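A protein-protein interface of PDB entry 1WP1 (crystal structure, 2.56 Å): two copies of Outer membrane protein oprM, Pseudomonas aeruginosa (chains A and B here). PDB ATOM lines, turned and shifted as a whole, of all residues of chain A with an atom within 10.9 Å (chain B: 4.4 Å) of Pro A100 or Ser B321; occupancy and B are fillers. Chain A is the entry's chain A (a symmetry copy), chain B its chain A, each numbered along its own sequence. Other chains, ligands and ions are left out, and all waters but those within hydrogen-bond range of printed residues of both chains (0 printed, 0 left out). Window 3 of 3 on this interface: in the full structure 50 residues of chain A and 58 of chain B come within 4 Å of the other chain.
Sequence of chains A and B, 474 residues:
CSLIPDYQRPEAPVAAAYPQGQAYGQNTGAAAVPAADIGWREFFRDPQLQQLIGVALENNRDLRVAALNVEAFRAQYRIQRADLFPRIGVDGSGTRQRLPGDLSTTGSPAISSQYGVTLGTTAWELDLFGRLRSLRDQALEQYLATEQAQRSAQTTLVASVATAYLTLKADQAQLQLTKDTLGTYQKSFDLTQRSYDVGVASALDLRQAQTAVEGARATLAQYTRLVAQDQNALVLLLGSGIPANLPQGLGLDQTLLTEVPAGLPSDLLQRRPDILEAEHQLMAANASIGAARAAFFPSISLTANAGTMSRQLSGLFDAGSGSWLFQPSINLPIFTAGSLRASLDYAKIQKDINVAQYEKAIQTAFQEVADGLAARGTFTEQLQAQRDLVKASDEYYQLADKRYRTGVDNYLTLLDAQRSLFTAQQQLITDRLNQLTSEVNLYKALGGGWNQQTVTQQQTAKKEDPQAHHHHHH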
ATOM      1  N   GLN A  97      -2.493 -27.665 -26.924  1.00  0.00           N
ATOM      2  CA  GLN A  97      -3.337 -26.700 -26.229  1.00  0.00           C
ATOM      3  C   GLN A  97      -4.707 -26.423 -26.857  1.00  0.00           C
ATOM      4  O   GLN A  97      -4.894 -26.525 -28.065  1.00  0.00           O
ATOM      5  CB  GLN A  97      -2.584 -25.392 -26.005  1.00  0.00           C
ATOM      6  CG  GLN A  97      -2.006 -24.749 -27.251  1.00  0.00           C
ATOM      7  CD  GLN A  97      -1.346 -23.403 -26.950  1.00  0.00           C
ATOM      8  OE1 GLN A  97      -1.530 -22.832 -25.867  1.00  0.00           O
ATOM      9  NE2 GLN A  97      -0.577 -22.891 -27.906  1.00  0.00           N
ATOM     10  N   ARG A  98      -5.669 -26.083 -26.011  1.00  0.00           N
ATOM     11  CA  ARG A  98      -6.917 -25.538 -26.484  1.00  0.00           C
ATOM     12  C   ARG A  98      -6.910 -24.034 -26.298  1.00  0.00           C
ATOM     13  O   ARG A  98      -6.715 -23.538 -25.191  1.00  0.00           O
ATOM     14  CB  ARG A  98      -8.110 -26.130 -25.749  1.00  0.00           C
ATOM     15  CG  ARG A  98      -9.423 -25.630 -26.313  1.00  0.00           C
ATOM     16  CD  ARG A  98     -10.605 -25.906 -25.418  1.00  0.00           C
ATOM     17  NE  ARG A  98     -11.510 -24.769 -25.481  1.00  0.00           N
ATOM     18  CZ  ARG A  98     -12.808 -24.814 -25.228  1.00  0.00           C
ATOM     19  NH1 ARG A  98     -13.390 -25.957 -24.894  1.00  0.00           N
ATOM     20  NH2 ARG A  98     -13.526 -23.704 -25.317  1.00  0.00           N
ATOM     21  N   LEU A  99      -7.141 -23.320 -27.394  1.00  0.00           N
ATOM     22  CA  LEU A  99      -7.212 -21.863 -27.390  1.00  0.00           C
ATOM     23  C   LEU A  99      -8.652 -21.398 -27.600  1.00  0.00           C
ATOM     24  O   LEU A  99      -9.486 -22.173 -28.067  1.00  0.00           O
ATOM     25  CB  LEU A  99      -6.276 -21.294 -28.471  1.00  0.00           C
ATOM     26  CG  LEU A  99      -4.780 -21.605 -28.306  1.00  0.00           C
ATOM     27  CD1 LEU A  99      -3.916 -20.914 -29.368  1.00  0.00           C
ATOM     28  CD2 LEU A  99      -4.312 -21.223 -26.908  1.00  0.00           C
ATOM     29  N   PRO A 100      -8.967 -20.142 -27.233  1.00  0.00           N
ATOM     30  CA  PRO A 100     -10.291 -19.636 -27.607  1.00  0.00           C
ATOM     31  C   PRO A 100     -10.330 -19.091 -29.046  1.00  0.00           C
ATOM     32  O   PRO A 100      -9.279 -18.977 -29.701  1.00  0.00           O
ATOM     33  CB  PRO A 100     -10.557 -18.526 -26.580  1.00  0.00           C
ATOM     34  CG  PRO A 100      -9.234 -18.213 -25.947  1.00  0.00           C
ATOM     35  CD  PRO A 100      -8.187 -19.147 -26.477  1.00  0.00           C
ATOM     36  N   GLY A 101     -11.538 -18.771 -29.521  1.00  0.00           N
ATOM     37  CA  GLY A 101     -11.758 -18.304 -30.889  1.00  0.00           C
ATOM     38  C   GLY A 101     -10.943 -17.086 -31.271  1.00  0.00           C
ATOM     39  O   GLY A 101     -10.394 -17.009 -32.374  1.00  0.00           O
ATOM     40  N   ASP A 102     -10.853 -16.137 -30.345  1.00  0.00           N
ATOM     41  CA  ASP A 102     -10.094 -14.913 -30.576  1.00  0.00           C
ATOM     42  C   ASP A 102      -8.559 -15.101 -30.555  1.00  0.00           C
ATOM     43  O   ASP A 102      -7.805 -14.149 -30.754  1.00  0.00           O
ATOM     44  CB  ASP A 102     -10.569 -13.779 -29.644  1.00  0.00           C
ATOM     45  CG  ASP A 102     -10.277 -14.032 -28.147  1.00  0.00           C
ATOM     46  OD1 ASP A 102      -9.925 -15.162 -27.729  1.00  0.00           O
ATOM     47  OD2 ASP A 102     -10.414 -13.066 -27.366  1.00  0.00           O
ATOM     48  N   LEU A 103      -8.101 -16.325 -30.317  1.00  0.00           N
ATOM     49  CA  LEU A 103      -6.672 -16.617 -30.405  1.00  0.00           C
ATOM     50  C   LEU A 103      -6.363 -17.733 -31.410  1.00  0.00           C
ATOM     51  O   LEU A 103      -5.270 -17.789 -31.946  1.00  0.00           O
ATOM     52  CB  LEU A 103      -6.074 -16.920 -29.022  1.00  0.00           C
ATOM     53  CG  LEU A 103      -6.013 -15.748 -28.031  1.00  0.00           C
ATOM     54  CD1 LEU A 103      -5.718 -16.224 -26.621  1.00  0.00           C
ATOM     55  CD2 LEU A 103      -5.004 -14.681 -28.445  1.00  0.00           C
ATOM     56  N   SER A 104      -7.342 -18.588 -31.688  1.00  0.00           N
ATOM     57  CA  SER A 104      -7.146 -19.731 -32.580  1.00  0.00           C
ATOM     58  C   SER A 104      -6.865 -19.352 -34.036  1.00  0.00           C
ATOM     59  O   SER A 104      -7.066 -18.203 -34.440  1.00  0.00           O
ATOM     60  CB  SER A 104      -8.355 -20.657 -32.517  1.00  0.00           C
ATOM     61  OG  SER A 104      -9.540 -19.971 -32.888  1.00  0.00           O
ATOM     62  N   THR A 105      -6.389 -20.329 -34.807  1.00  0.00           N
ATOM     63  CA  THR A 105      -6.202 -20.207 -36.261  1.00  0.00           C
ATOM     64  C   THR A 105      -7.549 -20.117 -37.003  1.00  0.00           C
ATOM     65  O   THR A 105      -7.656 -19.449 -38.035  1.00  0.00           O
ATOM     66  CB  THR A 105      -5.404 -21.421 -36.854  1.00  0.00           C
ATOM     67  OG1 THR A 105      -6.038 -22.649 -36.478  1.00  0.00           O
ATOM     68  CG2 THR A 105      -3.969 -21.446 -36.363  1.00  0.00           C
ATOM     69  N   THR A 106      -8.567 -20.797 -36.478  1.00  0.00           N
ATOM     70  CA  THR A 106      -9.858 -20.873 -37.138  1.00  0.00           C
ATOM     71  C   THR A 106     -10.689 -19.601 -36.887  1.00  0.00           C
ATOM     72  O   THR A 106     -11.160 -18.957 -37.836  1.00  0.00           O
ATOM     73  CB  THR A 106     -10.625 -22.186 -36.772  1.00  0.00           C
ATOM     74  OG1 THR A 106     -11.187 -22.105 -35.452  1.00  0.00           O
ATOM     75  CG2 THR A 106      -9.690 -23.395 -36.855  1.00  0.00           C
ATOM     76  N   GLY A 107     -10.847 -19.228 -35.619  1.00  0.00           N
ATOM     77  CA  GLY A 107     -11.734 -18.129 -35.237  1.00  0.00           C
ATOM     78  C   GLY A 107     -12.814 -18.637 -34.307  1.00  0.00           C
ATOM     79  O   GLY A 107     -13.547 -17.853 -33.705  1.00  0.00           O
ATOM     80  N   SER A 108     -12.934 -19.956 -34.215  1.00  0.00           N
ATOM     81  CA  SER A 108     -13.682 -20.579 -33.129  1.00  0.00           C
ATOM     82  C   SER A 108     -12.742 -21.473 -32.289  1.00  0.00           C
ATOM     83  O   SER A 108     -11.638 -21.808 -32.740  1.00  0.00           O
ATOM     84  CB  SER A 108     -14.930 -21.316 -33.644  1.00  0.00           C
ATOM     85  OG  SER A 108     -14.621 -22.211 -34.688  1.00  0.00           O
ATOM     86  N   PRO A 109     -13.152 -21.820 -31.051  1.00  0.00           N
ATOM     87  CA  PRO A 109     -12.294 -22.589 -30.145  1.00  0.00           C
ATOM     88  C   PRO A 109     -11.664 -23.840 -30.766  1.00  0.00           C
ATOM     89  O   PRO A 109     -12.345 -24.826 -31.014  1.00  0.00           O
ATOM     90  CB  PRO A 109     -13.247 -22.960 -29.006  1.00  0.00           C
ATOM     91  CG  PRO A 109     -14.223 -21.833 -28.971  1.00  0.00           C
ATOM     92  CD  PRO A 109     -14.447 -21.492 -30.417  1.00  0.00           C
ATOM     93  N   ALA A 110     -10.356 -23.780 -30.994  1.00  0.00           N
ATOM     94  CA  ALA A 110      -9.586 -24.858 -31.631  1.00  0.00           C
ATOM     95  C   ALA A 110      -8.598 -25.602 -30.687  1.00  0.00           C
ATOM     96  O   ALA A 110      -8.287 -25.128 -29.589  1.00  0.00           O
ATOM     97  CB  ALA A 110      -8.829 -24.295 -32.840  1.00  0.00           C
ATOM     98  N   ILE A 111      -8.119 -26.764 -31.135  1.00  0.00           N
ATOM     99  CA  ILE A 111      -7.144 -27.556 -30.402  1.00  0.00           C
ATOM    100  C   ILE A 111      -5.923 -27.786 -31.291  1.00  0.00           C
ATOM    101  O   ILE A 111      -5.919 -28.675 -32.131  1.00  0.00           O
ATOM    102  CB  ILE A 111      -7.741 -28.902 -29.897  1.00  0.00           C
ATOM    103  CG1 ILE A 111      -8.962 -28.638 -29.008  1.00  0.00           C
ATOM    104  CG2 ILE A 111      -6.696 -29.699 -29.120  1.00  0.00           C
ATOM    105  CD1 ILE A 111      -9.649 -29.894 -28.430  1.00  0.00           C
ATOM    106  N   SER A 112      -4.899 -26.958 -31.119  1.00  0.00           N
ATOM    107  CA  SER A 112      -3.672 -27.100 -31.880  1.00  0.00           C
ATOM    108  C   SER A 112      -2.723 -27.993 -31.096  1.00  0.00           C
ATOM    109  O   SER A 112      -3.010 -28.325 -29.941  1.00  0.00           O
ATOM    110  CB  SER A 112      -3.044 -25.738 -32.137  1.00  0.00           C
ATOM    111  OG  SER A 112      -2.686 -25.118 -30.922  1.00  0.00           O
ATOM    112  N   THR B 308      -8.593 -19.409 -18.448  1.00  0.00           N
ATOM    113  CA  THR B 308      -9.279 -18.579 -19.433  1.00  0.00           C
ATOM    114  C   THR B 308      -8.272 -17.658 -20.109  1.00  0.00           C
ATOM    115  O   THR B 308      -7.627 -16.855 -19.442  1.00  0.00           O
ATOM    116  CB  THR B 308     -10.433 -17.731 -18.802  1.00  0.00           C
ATOM    117  OG1 THR B 308      -9.912 -16.856 -17.791  1.00  0.00           O
ATOM    118  CG2 THR B 308     -11.546 -18.621 -18.193  1.00  0.00           C
ATOM    119  N   MET B 309      -8.122 -17.799 -21.425  1.00  0.00           N
ATOM    120  CA  MET B 309      -7.256 -16.918 -22.225  1.00  0.00           C
ATOM    121  C   MET B 309      -8.084 -15.964 -23.095  1.00  0.00           C
ATOM    122  O   MET B 309      -9.269 -16.208 -23.345  1.00  0.00           O
ATOM    123  CB  MET B 309      -6.316 -17.738 -23.114  1.00  0.00           C
ATOM    124  CG  MET B 309      -5.114 -18.334 -22.401  1.00  0.00           C
ATOM    125  SD  MET B 309      -4.060 -19.348 -23.477  1.00  0.00           S
ATOM    126  CE  MET B 309      -3.006 -18.100 -24.221  1.00  0.00           C
ATOM    127  N   GLY B 315     -11.988  -9.978 -22.093  1.00  0.00           N
ATOM    128  CA  GLY B 315     -12.651 -11.198 -22.521  1.00  0.00           C
ATOM    129  C   GLY B 315     -12.321 -12.417 -21.692  1.00  0.00           C
ATOM    130  O   GLY B 315     -12.780 -13.518 -22.005  1.00  0.00           O
ATOM    131  N   LEU B 316     -11.542 -12.213 -20.628  1.00  0.00           N
ATOM    132  CA  LEU B 316     -11.059 -13.304 -19.758  1.00  0.00           C
ATOM    133  C   LEU B 316     -12.145 -14.175 -19.123  1.00  0.00           C
ATOM    134  O   LEU B 316     -12.209 -15.371 -19.384  1.00  0.00           O
ATOM    135  CB  LEU B 316     -10.134 -12.769 -18.663  1.00  0.00           C
ATOM    136  CG  LEU B 316      -8.663 -12.502 -18.985  1.00  0.00           C
ATOM    137  CD1 LEU B 316      -8.021 -11.897 -17.753  1.00  0.00           C
ATOM    138  CD2 LEU B 316      -7.919 -13.745 -19.404  1.00  0.00           C
ATOM    139  N   ASP B 318     -15.242 -14.466 -19.699  1.00  0.00           N
ATOM    140  CA  ASP B 318     -16.399 -14.499 -20.567  1.00  0.00           C
ATOM    141  C   ASP B 318     -16.504 -15.916 -21.098  1.00  0.00           C
ATOM    142  O   ASP B 318     -15.496 -16.595 -21.268  1.00  0.00           O
ATOM    143  CB  ASP B 318     -16.239 -13.501 -21.714  1.00  0.00           C
ATOM    144  CG  ASP B 318     -17.569 -13.058 -22.294  1.00  0.00           C
ATOM    145  OD1 ASP B 318     -18.238 -13.871 -22.969  1.00  0.00           O
ATOM    146  OD2 ASP B 318     -17.938 -11.883 -22.079  1.00  0.00           O
ATOM    147  N   ALA B 319     -17.734 -16.350 -21.343  1.00  0.00           N
ATOM    148  CA  ALA B 319     -18.034 -17.711 -21.783  1.00  0.00           C
ATOM    149  C   ALA B 319     -17.151 -18.174 -22.933  1.00  0.00           C
ATOM    150  O   ALA B 319     -16.757 -17.374 -23.786  1.00  0.00           O
ATOM    151  CB  ALA B 319     -19.514 -17.819 -22.173  1.00  0.00           C
ATOM    152  N   GLY B 320     -16.835 -19.465 -22.937  1.00  0.00           N
ATOM    153  CA  GLY B 320     -16.088 -20.089 -24.034  1.00  0.00           C
ATOM    154  C   GLY B 320     -14.753 -19.441 -24.358  1.00  0.00           C
ATOM    155  O   GLY B 320     -14.279 -19.520 -25.496  1.00  0.00           O
ATOM    156  N   SER B 321     -14.159 -18.779 -23.366  1.00  0.00           N
ATOM    157  CA  SER B 321     -12.793 -18.277 -23.484  1.00  0.00           C
ATOM    158  C   SER B 321     -11.867 -19.298 -22.840  1.00  0.00           C
ATOM    159  O   SER B 321     -10.659 -19.078 -22.725  1.00  0.00           O
ATOM    160  CB  SER B 321     -12.638 -16.901 -22.824  1.00  0.00           C
ATOM    161  OG  SER B 321     -12.965 -16.951 -21.450  1.00  0.00           O
ATOM    162  N   GLY B 322     -12.457 -20.420 -22.430  1.00  0.00           N
ATOM    163  CA  GLY B 322     -11.732 -21.533 -21.826  1.00  0.00           C
ATOM    164  C   GLY B 322     -10.462 -21.862 -22.580  1.00  0.00           C
ATOM    165  O   GLY B 322     -10.429 -21.792 -23.810  1.00  0.00           O
ATOM    166  N   SER B 323      -9.416 -22.197 -21.824  1.00  0.00           N
ATOM    167  CA  SER B 323      -8.109 -22.573 -22.366  1.00  0.00           C
ATOM    168  C   SER B 323      -7.492 -23.667 -21.529  1.00  0.00           C
ATOM    169  O   SER B 323      -7.786 -23.781 -20.340  1.00  0.00           O
ATOM    170  CB  SER B 323      -7.170 -21.371 -22.365  1.00  0.00           C
ATOM    171  OG  SER B 323      -7.258 -20.666 -21.135  1.00  0.00           O
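The backbone NH of Met B309 sits at hydrogen-bond distance from the backbone carbonyl oxygen of Ser B321 (3.1 Å). The side-chain hydroxyl (OG) of Ser B321 lies within hydrogen-bond range of the backbone carbonyl oxygen (O) of Asp B318. N of Met B309 sits at hydrogen-bond distance from OG of Ser B323 (3.0 Å). The side-chain hydroxyl (OG) of Ser B323 is in hydrogen-bond range of the backbone NH (N) of Thr B308. The backbone NH (N) of Leu A99 lies within hydrogen-bond range of the backbone carbonyl oxygen (O) of Ala A110 (3.1 Å). The side-chain hydroxyl (OG) of Ser B321 is in hydrogen-bond range of the backbone carbonyl oxygen (O) of Leu B316 (2.7 Å).
Among the printed residues, merely in contact across the chains: Pro A100 with Met B309, Arg A98 with Ser B323, Arg A98 with Gly B322, Pro A100 with Ser B321, Leu A103 with Met B309 and Leu A99 with Met B309.
Of the printed residues of chain B, Pro A100 touches Met B309 (3.3 Å) and Ser B321 (3.6 Å). Ser B321 touches just one residue of chain A: Pro A100. No residue of chain A comes within 4 Å of Thr B308. No residue of chain A comes within 4 Å of Ala B319. Gly B322 touches just one residue of chain A: Arg A98 (3.6 Å). Ser B323 touches just one residue of chain A: Arg A98. Printed residues of chain B within 4 Å of Arg A98: Gly B322 and Ser B323. Of the printed residues of chain B, Leu A99 touches Met B309. Printed residues of chain B within 4 Å of Leu A103: Met B309 (3.9 Å). The nearest printed residue of chain B that does not touch Pro A100 is Gly B320 (4.002 Å). The nearest residue of chain A that does not touch Ser B321 is Arg A98 (5.3 Å). The nearest printed residue of chain B that does not touch Arg A98 is Gly B320 (4.3 Å).
Of the 16 printed residues of chain A, 4 touch a printed residue of chain B. Printed residues of chain A that touch a printed residue of chain B: Arg A98, Leu A99, Pro A100 and Leu A103. Hydrophobic or aromatic side chains of chain A that line the printed part of chain B: Leu A99, Pro A100 and Leu A103. Hydrophobic or aromatic side chains of chain B within 4 Å of the printed part of chain A: Met B309. Among the printed residues, no Asp or Glu carboxylate lies within 4 Å of a Lys or Arg side-chain nitrogen of the other chain.
No position is printed for both chains.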
